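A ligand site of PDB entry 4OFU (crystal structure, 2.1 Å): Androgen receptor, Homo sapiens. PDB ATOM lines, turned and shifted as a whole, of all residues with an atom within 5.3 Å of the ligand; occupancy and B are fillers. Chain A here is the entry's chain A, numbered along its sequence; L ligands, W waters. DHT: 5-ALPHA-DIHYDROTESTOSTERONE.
The side-chain hydroxyl (OG1) of Thr 208 sits at hydrogen-bond distance from an oxygen (O17) of the ligand, at 2.6 Å.
The side-chain amide oxygen (OD1) of Asn 36 is in hydrogen-bond range of an oxygen (O17) of the ligand, at 2.7 Å.
The guanidinium group (NH2) of Arg 83 lies within hydrogen-bond range of an oxygen (O3) of the ligand (2.9 Å).
O3 of the ligand sits close to OE1 of Gln 42 (3.4 Å).
The backbone carbonyl oxygen of Leu 32 sits close to the side-chain amide nitrogen of Asn 36 (3.5 Å).
OE1 of Gln 42 is in hydrogen-bond range of NH2 of Arg 83 (3.4 Å).
NH2 of Arg 83 sits at hydrogen-bond distance from O of Phe 95 (2.9 Å).
The side-chain sulfur (SD) of Met 76 lies close to the side-chain amide nitrogen (NE2) of Gln 42, at 3.7 Å.
Water W1 lies within hydrogen-bond range of the side-chain amide nitrogen (NE2) of Gln 42 (2.5 Å), the backbone carbonyl oxygen (O) of Met 76 (2.9 Å), the guanidinium group (NH2) of Arg 83 (2.9 Å) and an oxygen (O3) of the ligand (3.2 Å).
Leu 32 touches the ligand (CD1 to C17, 3.8 Å).
O of Leu 35 touches C11 of the ligand (3.3 Å).
CE of Met 73 touches C18 of the ligand, at 3.9 Å.
Met 76 touches the ligand.
CG2 of Val 77 touches C6 of the ligand (3.98 Å).
CB of Met 80 touches O3 of the ligand, 3.6 Å away.
Phe 95 touches the ligand.
Leu 204 touches the ligand.
CD1 of Phe 207 touches C16 of the ligand (3.9 Å).
CE2 of Phe 222 touches O17 of the ligand, 3.8 Å away.
Met 226 touches the ligand (CE to C12, 3.9 Å).
15 residues have an atom within 4 Å of the ligand: Leu 32, Leu 35, Asn 36, Gln 42, Met 73, Met 76, Val 77, Met 80, Arg 83, Phe 95, Leu 204, Phe 207, Thr 208, Phe 222 and Met 226.
The nearest printed residue that does not touch the ligand is Met 111 (4.04 Å).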
ATOM      1  N   LEU A  32       2.213  13.160  -1.352  1.00  0.00           N
ATOM      2  CA  LEU A  32       2.413  12.738   0.012  1.00  0.00           C
ATOM      3  C   LEU A  32       2.638  11.248   0.139  1.00  0.00           C
ATOM      4  O   LEU A  32       3.498  10.845   0.912  1.00  0.00           O
ATOM      5  CB  LEU A  32       1.355  13.304   0.972  1.00  0.00           C
ATOM      6  CG  LEU A  32       1.844  14.630   1.595  1.00  0.00           C
ATOM      7  CD1 LEU A  32       3.058  14.493   2.536  1.00  0.00           C
ATOM      8  CD2 LEU A  32       2.092  15.707   0.547  1.00  0.00           C
ATOM      9  N   LEU A  35       6.143  10.459  -0.887  1.00  0.00           N
ATOM     10  CA  LEU A  35       7.133  10.928   0.106  1.00  0.00           C
ATOM     11  C   LEU A  35       7.166   9.941   1.264  1.00  0.00           C
ATOM     12  O   LEU A  35       8.205   9.573   1.839  1.00  0.00           O
ATOM     13  CB  LEU A  35       6.803  12.324   0.618  1.00  0.00           C
ATOM     14  CG  LEU A  35       7.270  13.547  -0.182  1.00  0.00           C
ATOM     15  CD1 LEU A  35       6.650  14.771   0.457  1.00  0.00           C
ATOM     16  CD2 LEU A  35       8.797  13.722  -0.175  1.00  0.00           C
ATOM     17  N   ASN A  36       5.993   9.480   1.622  1.00  0.00           N
ATOM     18  CA  ASN A  36       5.919   8.465   2.666  1.00  0.00           C
ATOM     19  C   ASN A  36       6.633   7.220   2.254  1.00  0.00           C
ATOM     20  O   ASN A  36       7.304   6.567   3.072  1.00  0.00           O
ATOM     21  CB  ASN A  36       4.475   8.134   3.001  1.00  0.00           C
ATOM     22  CG  ASN A  36       3.823   9.220   3.832  1.00  0.00           C
ATOM     23  OD1 ASN A  36       4.509  10.049   4.500  1.00  0.00           O
ATOM     24  ND2 ASN A  36       2.501   9.221   3.814  1.00  0.00           N
ATOM     25  N   LEU A  38       9.162   7.082   0.011  1.00  0.00           N
ATOM     26  CA  LEU A  38      10.597   7.507   0.148  1.00  0.00           C
ATOM     27  C   LEU A  38      11.081   7.347   1.581  1.00  0.00           C
ATOM     28  O   LEU A  38      12.181   6.799   1.846  1.00  0.00           O
ATOM     29  CB  LEU A  38      10.830   8.962  -0.389  1.00  0.00           C
ATOM     30  CG  LEU A  38      12.312   9.347  -0.492  1.00  0.00           C
ATOM     31  CD1 LEU A  38      13.056   8.309  -1.355  1.00  0.00           C
ATOM     32  CD2 LEU A  38      12.460  10.733  -1.110  1.00  0.00           C
ATOM     33  N   GLY A  39      10.270   7.751   2.538  1.00  0.00           N
ATOM     34  CA  GLY A  39      10.710   7.624   3.932  1.00  0.00           C
ATOM     35  C   GLY A  39      10.980   6.188   4.403  1.00  0.00           C
ATOM     36  O   GLY A  39      11.900   5.926   5.169  1.00  0.00           O
ATOM     37  N   GLN A  42      14.134   5.114   2.757  1.00  0.00           N
ATOM     38  CA  GLN A  42      15.319   5.758   3.332  1.00  0.00           C
ATOM     39  C   GLN A  42      15.504   5.259   4.731  1.00  0.00           C
ATOM     40  O   GLN A  42      16.626   5.135   5.188  1.00  0.00           O
ATOM     41  CB  GLN A  42      15.165   7.266   3.296  1.00  0.00           C
ATOM     42  CG  GLN A  42      15.234   7.832   1.884  1.00  0.00           C
ATOM     43  CD  GLN A  42      15.694   9.311   1.854  1.00  0.00           C
ATOM     44  OE1 GLN A  42      15.675   9.999   0.810  1.00  0.00           O
ATOM     45  NE2 GLN A  42      16.139   9.785   3.009  1.00  0.00           N
ATOM     46  N   TRP A  72      15.492  10.239  12.659  1.00  0.00           N
ATOM     47  CA  TRP A  72      15.491  10.013  11.203  1.00  0.00           C
ATOM     48  C   TRP A  72      14.994  11.202  10.427  1.00  0.00           C
ATOM     49  O   TRP A  72      15.458  11.441   9.359  1.00  0.00           O
ATOM     50  CB  TRP A  72      14.646   8.752  10.764  1.00  0.00           C
ATOM     51  CG  TRP A  72      13.186   8.863  11.256  1.00  0.00           C
ATOM     52  CD1 TRP A  72      12.721   8.502  12.486  1.00  0.00           C
ATOM     53  CD2 TRP A  72      12.073   9.438  10.571  1.00  0.00           C
ATOM     54  NE1 TRP A  72      11.365   8.834  12.626  1.00  0.00           N
ATOM     55  CE2 TRP A  72      10.947   9.361  11.427  1.00  0.00           C
ATOM     56  CE3 TRP A  72      11.910   9.999   9.289  1.00  0.00           C
ATOM     57  CZ2 TRP A  72       9.690   9.832  11.039  1.00  0.00           C
ATOM     58  CZ3 TRP A  72      10.641  10.454   8.900  1.00  0.00           C
ATOM     59  CH2 TRP A  72       9.561  10.357   9.763  1.00  0.00           C
ATOM     60  N   MET A  73      14.015  11.951  10.952  1.00  0.00           N
ATOM     61  CA  MET A  73      13.560  13.129  10.269  1.00  0.00           C
ATOM     62  C   MET A  73      14.664  14.170  10.016  1.00  0.00           C
ATOM     63  O   MET A  73      14.797  14.635   8.884  1.00  0.00           O
ATOM     64  CB  MET A  73      12.448  13.879  11.067  1.00  0.00           C
ATOM     65  CG  MET A  73      11.753  14.907  10.213  1.00  0.00           C
ATOM     66  SD  MET A  73      10.660  14.426   8.847  1.00  0.00           S
ATOM     67  CE  MET A  73       9.240  13.899   9.809  1.00  0.00           C
ATOM     68  N   MET A  76      17.363  12.663   7.613  1.00  0.00           N
ATOM     69  CA  MET A  76      16.929  12.712   6.222  1.00  0.00           C
ATOM     70  C   MET A  76      16.763  14.131   5.655  1.00  0.00           C
ATOM     71  O   MET A  76      16.992  14.372   4.480  1.00  0.00           O
ATOM     72  CB  MET A  76      15.570  11.976   6.075  1.00  0.00           C
ATOM     73  CG  MET A  76      15.678  10.542   6.569  1.00  0.00           C
ATOM     74  SD  MET A  76      14.186   9.586   6.192  1.00  0.00           S
ATOM     75  CE  MET A  76      14.761   8.072   6.976  1.00  0.00           C
ATOM     76  N   VAL A  77      16.265  15.049   6.451  1.00  0.00           N
ATOM     77  CA  VAL A  77      16.104  16.424   5.935  1.00  0.00           C
ATOM     78  C   VAL A  77      17.457  17.013   5.618  1.00  0.00           C
ATOM     79  O   VAL A  77      17.594  17.627   4.595  1.00  0.00           O
ATOM     80  CB  VAL A  77      15.345  17.329   6.928  1.00  0.00           C
ATOM     81  CG1 VAL A  77      15.571  18.821   6.613  1.00  0.00           C
ATOM     82  CG2 VAL A  77      13.879  16.980   6.877  1.00  0.00           C
ATOM     83  N   MET A  80      18.855  15.575   2.377  1.00  0.00           N
ATOM     84  CA  MET A  80      18.123  16.001   1.215  1.00  0.00           C
ATOM     85  C   MET A  80      18.534  17.463   0.880  1.00  0.00           C
ATOM     86  O   MET A  80      18.609  17.872  -0.283  1.00  0.00           O
ATOM     87  CB  MET A  80      16.640  15.967   1.549  1.00  0.00           C
ATOM     88  CG  MET A  80      15.794  16.341   0.370  1.00  0.00           C
ATOM     89  SD  MET A  80      15.273  18.072   0.135  1.00  0.00           S
ATOM     90  CE  MET A  80      14.570  18.452   1.736  1.00  0.00           C
ATOM     91  N   ARG A  83      21.839  17.036  -1.016  1.00  0.00           N
ATOM     92  CA  ARG A  83      21.445  16.626  -2.386  1.00  0.00           C
ATOM     93  C   ARG A  83      20.900  17.801  -3.181  1.00  0.00           C
ATOM     94  O   ARG A  83      21.295  18.009  -4.323  1.00  0.00           O
ATOM     95  CB  ARG A  83      20.336  15.557  -2.381  1.00  0.00           C
ATOM     96  CG  ARG A  83      20.683  14.250  -1.735  1.00  0.00           C
ATOM     97  CD  ARG A  83      19.776  13.101  -2.256  1.00  0.00           C
ATOM     98  NE  ARG A  83      18.424  13.190  -1.680  1.00  0.00           N
ATOM     99  CZ  ARG A  83      18.126  12.954  -0.406  1.00  0.00           C
ATOM    100  NH1 ARG A  83      19.088  12.618   0.476  1.00  0.00           N
ATOM    101  NH2 ARG A  83      16.863  13.078   0.020  1.00  0.00           N
ATOM    102  N   PHE A  95      14.288  15.524  -3.212  1.00  0.00           N
ATOM    103  CA  PHE A  95      13.956  14.387  -2.356  1.00  0.00           C
ATOM    104  C   PHE A  95      14.544  13.105  -2.901  1.00  0.00           C
ATOM    105  O   PHE A  95      15.137  12.352  -2.143  1.00  0.00           O
ATOM    106  CB  PHE A  95      12.460  14.276  -2.193  1.00  0.00           C
ATOM    107  CG  PHE A  95      11.885  15.396  -1.405  1.00  0.00           C
ATOM    108  CD1 PHE A  95      11.102  16.358  -2.018  1.00  0.00           C
ATOM    109  CD2 PHE A  95      12.135  15.491  -0.044  1.00  0.00           C
ATOM    110  CE1 PHE A  95      10.557  17.401  -1.293  1.00  0.00           C
ATOM    111  CE2 PHE A  95      11.580  16.526   0.716  1.00  0.00           C
ATOM    112  CZ  PHE A  95      10.788  17.484   0.071  1.00  0.00           C
ATOM    113  N   MET A 111       2.691  21.811   2.130  1.00  0.00           N
ATOM    114  CA  MET A 111       3.791  21.900   3.087  1.00  0.00           C
ATOM    115  C   MET A 111       4.672  23.044   2.724  1.00  0.00           C
ATOM    116  O   MET A 111       5.897  22.955   2.888  1.00  0.00           O
ATOM    117  CB  MET A 111       4.673  20.686   2.982  1.00  0.00           C
ATOM    118  CG  MET A 111       4.000  19.379   3.220  1.00  0.00           C
ATOM    119  SD  MET A 111       5.247  18.316   3.933  1.00  0.00           S
ATOM    120  CE  MET A 111       6.375  18.011   2.571  1.00  0.00           C
ATOM    121  N   MET A 118      13.261  24.136   4.343  1.00  0.00           N
ATOM    122  CA  MET A 118      14.257  23.152   3.851  1.00  0.00           C
ATOM    123  C   MET A 118      15.133  23.742   2.727  1.00  0.00           C
ATOM    124  O   MET A 118      16.383  23.562   2.710  1.00  0.00           O
ATOM    125  CB  MET A 118      13.557  21.865   3.387  1.00  0.00           C
ATOM    126  CG  MET A 118      12.746  21.228   4.512  1.00  0.00           C
ATOM    127  SD  MET A 118      12.229  19.520   4.207  1.00  0.00           S
ATOM    128  CE  MET A 118      10.578  19.783   3.575  1.00  0.00           C
ATOM    129  N   LEU A 204       7.920  19.109  10.760  1.00  0.00           N
ATOM    130  CA  LEU A 204       7.569  18.045   9.899  1.00  0.00           C
ATOM    131  C   LEU A 204       6.915  16.929  10.703  1.00  0.00           C
ATOM    132  O   LEU A 204       6.044  16.244  10.188  1.00  0.00           O
ATOM    133  CB  LEU A 204       8.785  17.549   9.151  1.00  0.00           C
ATOM    134  CG  LEU A 204       9.254  18.486   8.038  1.00  0.00           C
ATOM    135  CD1 LEU A 204      10.480  17.902   7.391  1.00  0.00           C
ATOM    136  CD2 LEU A 204       8.206  18.799   6.945  1.00  0.00           C
ATOM    137  N   PHE A 207       3.555  17.973  11.361  1.00  0.00           N
ATOM    138  CA  PHE A 207       2.819  17.811  10.076  1.00  0.00           C
ATOM    139  C   PHE A 207       2.477  16.349   9.730  1.00  0.00           C
ATOM    140  O   PHE A 207       1.341  16.048   9.363  1.00  0.00           O
ATOM    141  CB  PHE A 207       3.556  18.478   8.913  1.00  0.00           C
ATOM    142  CG  PHE A 207       2.760  18.480   7.622  1.00  0.00           C
ATOM    143  CD1 PHE A 207       2.808  17.394   6.747  1.00  0.00           C
ATOM    144  CD2 PHE A 207       1.936  19.575   7.270  1.00  0.00           C
ATOM    145  CE1 PHE A 207       2.076  17.394   5.554  1.00  0.00           C
ATOM    146  CE2 PHE A 207       1.184  19.577   6.087  1.00  0.00           C
ATOM    147  CZ  PHE A 207       1.261  18.470   5.214  1.00  0.00           C
ATOM    148  N   THR A 208       3.467  15.461   9.837  1.00  0.00           N
ATOM    149  CA  THR A 208       3.268  14.047   9.471  1.00  0.00           C
ATOM    150  C   THR A 208       2.320  13.334  10.443  1.00  0.00           C
ATOM    151  O   THR A 208       1.484  12.479  10.068  1.00  0.00           O
ATOM    152  CB  THR A 208       4.626  13.272   9.339  1.00  0.00           C
ATOM    153  OG1 THR A 208       4.383  12.049   8.616  1.00  0.00           O
ATOM    154  CG2 THR A 208       5.264  12.972  10.690  1.00  0.00           C
ATOM    155  N   LEU A 211      -1.067  14.386   9.707  1.00  0.00           N
ATOM    156  CA  LEU A 211      -1.448  13.864   8.428  1.00  0.00           C
ATOM    157  C   LEU A 211      -1.860  12.392   8.565  1.00  0.00           C
ATOM    158  O   LEU A 211      -2.839  11.995   7.994  1.00  0.00           O
ATOM    159  CB  LEU A 211      -0.328  14.031   7.390  1.00  0.00           C
ATOM    160  CG  LEU A 211      -0.693  13.380   6.035  1.00  0.00           C
ATOM    161  CD1 LEU A 211      -1.885  14.001   5.308  1.00  0.00           C
ATOM    162  CD2 LEU A 211       0.489  13.325   5.107  1.00  0.00           C
ATOM    163  N   PHE A 222       0.492   5.534   4.233  1.00  0.00           N
ATOM    164  CA  PHE A 222       1.645   5.432   5.109  1.00  0.00           C
ATOM    165  C   PHE A 222       2.045   3.974   5.116  1.00  0.00           C
ATOM    166  O   PHE A 222       1.263   3.146   5.542  1.00  0.00           O
ATOM    167  CB  PHE A 222       1.296   5.868   6.548  1.00  0.00           C
ATOM    168  CG  PHE A 222       1.272   7.364   6.762  1.00  0.00           C
ATOM    169  CD1 PHE A 222       0.106   8.103   6.537  1.00  0.00           C
ATOM    170  CD2 PHE A 222       2.443   8.054   7.187  1.00  0.00           C
ATOM    171  CE1 PHE A 222       0.088   9.500   6.713  1.00  0.00           C
ATOM    172  CE2 PHE A 222       2.437   9.452   7.381  1.00  0.00           C
ATOM    173  CZ  PHE A 222       1.252  10.181   7.138  1.00  0.00           C
ATOM    174  N   MET A 226       6.748   3.416   8.950  1.00  0.00           N
ATOM    175  CA  MET A 226       6.393   4.824   9.019  1.00  0.00           C
ATOM    176  C   MET A 226       5.139   5.007   9.897  1.00  0.00           C
ATOM    177  O   MET A 226       5.164   5.820  10.803  1.00  0.00           O
ATOM    178  CB  MET A 226       6.242   5.436   7.601  1.00  0.00           C
ATOM    179  CG  MET A 226       7.597   5.553   6.847  1.00  0.00           C
ATOM    180  SD  MET A 226       8.685   6.965   7.400  1.00  0.00           S
ATOM    181  CE  MET A 226       7.805   8.279   6.580  1.00  0.00           C
ATOM    182  N   ILE A 230       5.488   6.892  13.520  1.00  0.00           N
ATOM    183  CA  ILE A 230       4.830   8.170  13.611  1.00  0.00           C
ATOM    184  C   ILE A 230       3.773   8.198  14.716  1.00  0.00           C
ATOM    185  O   ILE A 230       3.513   9.257  15.317  1.00  0.00           O
ATOM    186  CB  ILE A 230       4.331   8.657  12.225  1.00  0.00           C
ATOM    187  CG1 ILE A 230       5.555   8.817  11.290  1.00  0.00           C
ATOM    188  CG2 ILE A 230       3.493   9.949  12.340  1.00  0.00           C
ATOM    189  CD1 ILE A 230       5.202   9.036   9.813  1.00  0.00           C
HETATM  190  C1  DHT L   1      11.532  11.891   2.793  1.00  0.00           C
HETATM  191  C2  DHT L   1      13.036  11.659   2.901  1.00  0.00           C
HETATM  192  C3  DHT L   1      13.658  13.010   2.540  1.00  0.00           C
HETATM  193  O3  DHT L   1      14.431  13.099   1.573  1.00  0.00           O
HETATM  194  C4  DHT L   1      13.222  14.224   3.385  1.00  0.00           C
HETATM  195  C5  DHT L   1      11.677  14.223   3.528  1.00  0.00           C
HETATM  196  C6  DHT L   1      11.181  15.353   4.447  1.00  0.00           C
HETATM  197  C7  DHT L   1       9.652  15.350   4.618  1.00  0.00           C
HETATM  198  C8  DHT L   1       9.078  13.985   5.045  1.00  0.00           C
HETATM  199  C9  DHT L   1       9.521  12.860   4.081  1.00  0.00           C
HETATM  200  C10 DHT L   1      11.062  12.841   3.910  1.00  0.00           C
HETATM  201  C11 DHT L   1       8.885  11.477   4.494  1.00  0.00           C
HETATM  202  C12 DHT L   1       7.350  11.537   4.552  1.00  0.00           C
HETATM  203  C13 DHT L   1       6.860  12.701   5.425  1.00  0.00           C
HETATM  204  C14 DHT L   1       7.545  14.036   5.031  1.00  0.00           C
HETATM  205  C15 DHT L   1       6.785  15.101   5.842  1.00  0.00           C
HETATM  206  C16 DHT L   1       5.333  14.585   5.770  1.00  0.00           C
HETATM  207  C17 DHT L   1       5.399  13.118   5.239  1.00  0.00           C
HETATM  208  O17 DHT L   1       4.534  12.289   5.996  1.00  0.00           O
HETATM  209  C18 DHT L   1       7.171  12.439   6.903  1.00  0.00           C
HETATM  210  C19 DHT L   1      11.630  12.287   5.219  1.00  0.00           C
HETATM  211  O   HOH W   1      17.275  12.044   2.731  1.00  0.00           O
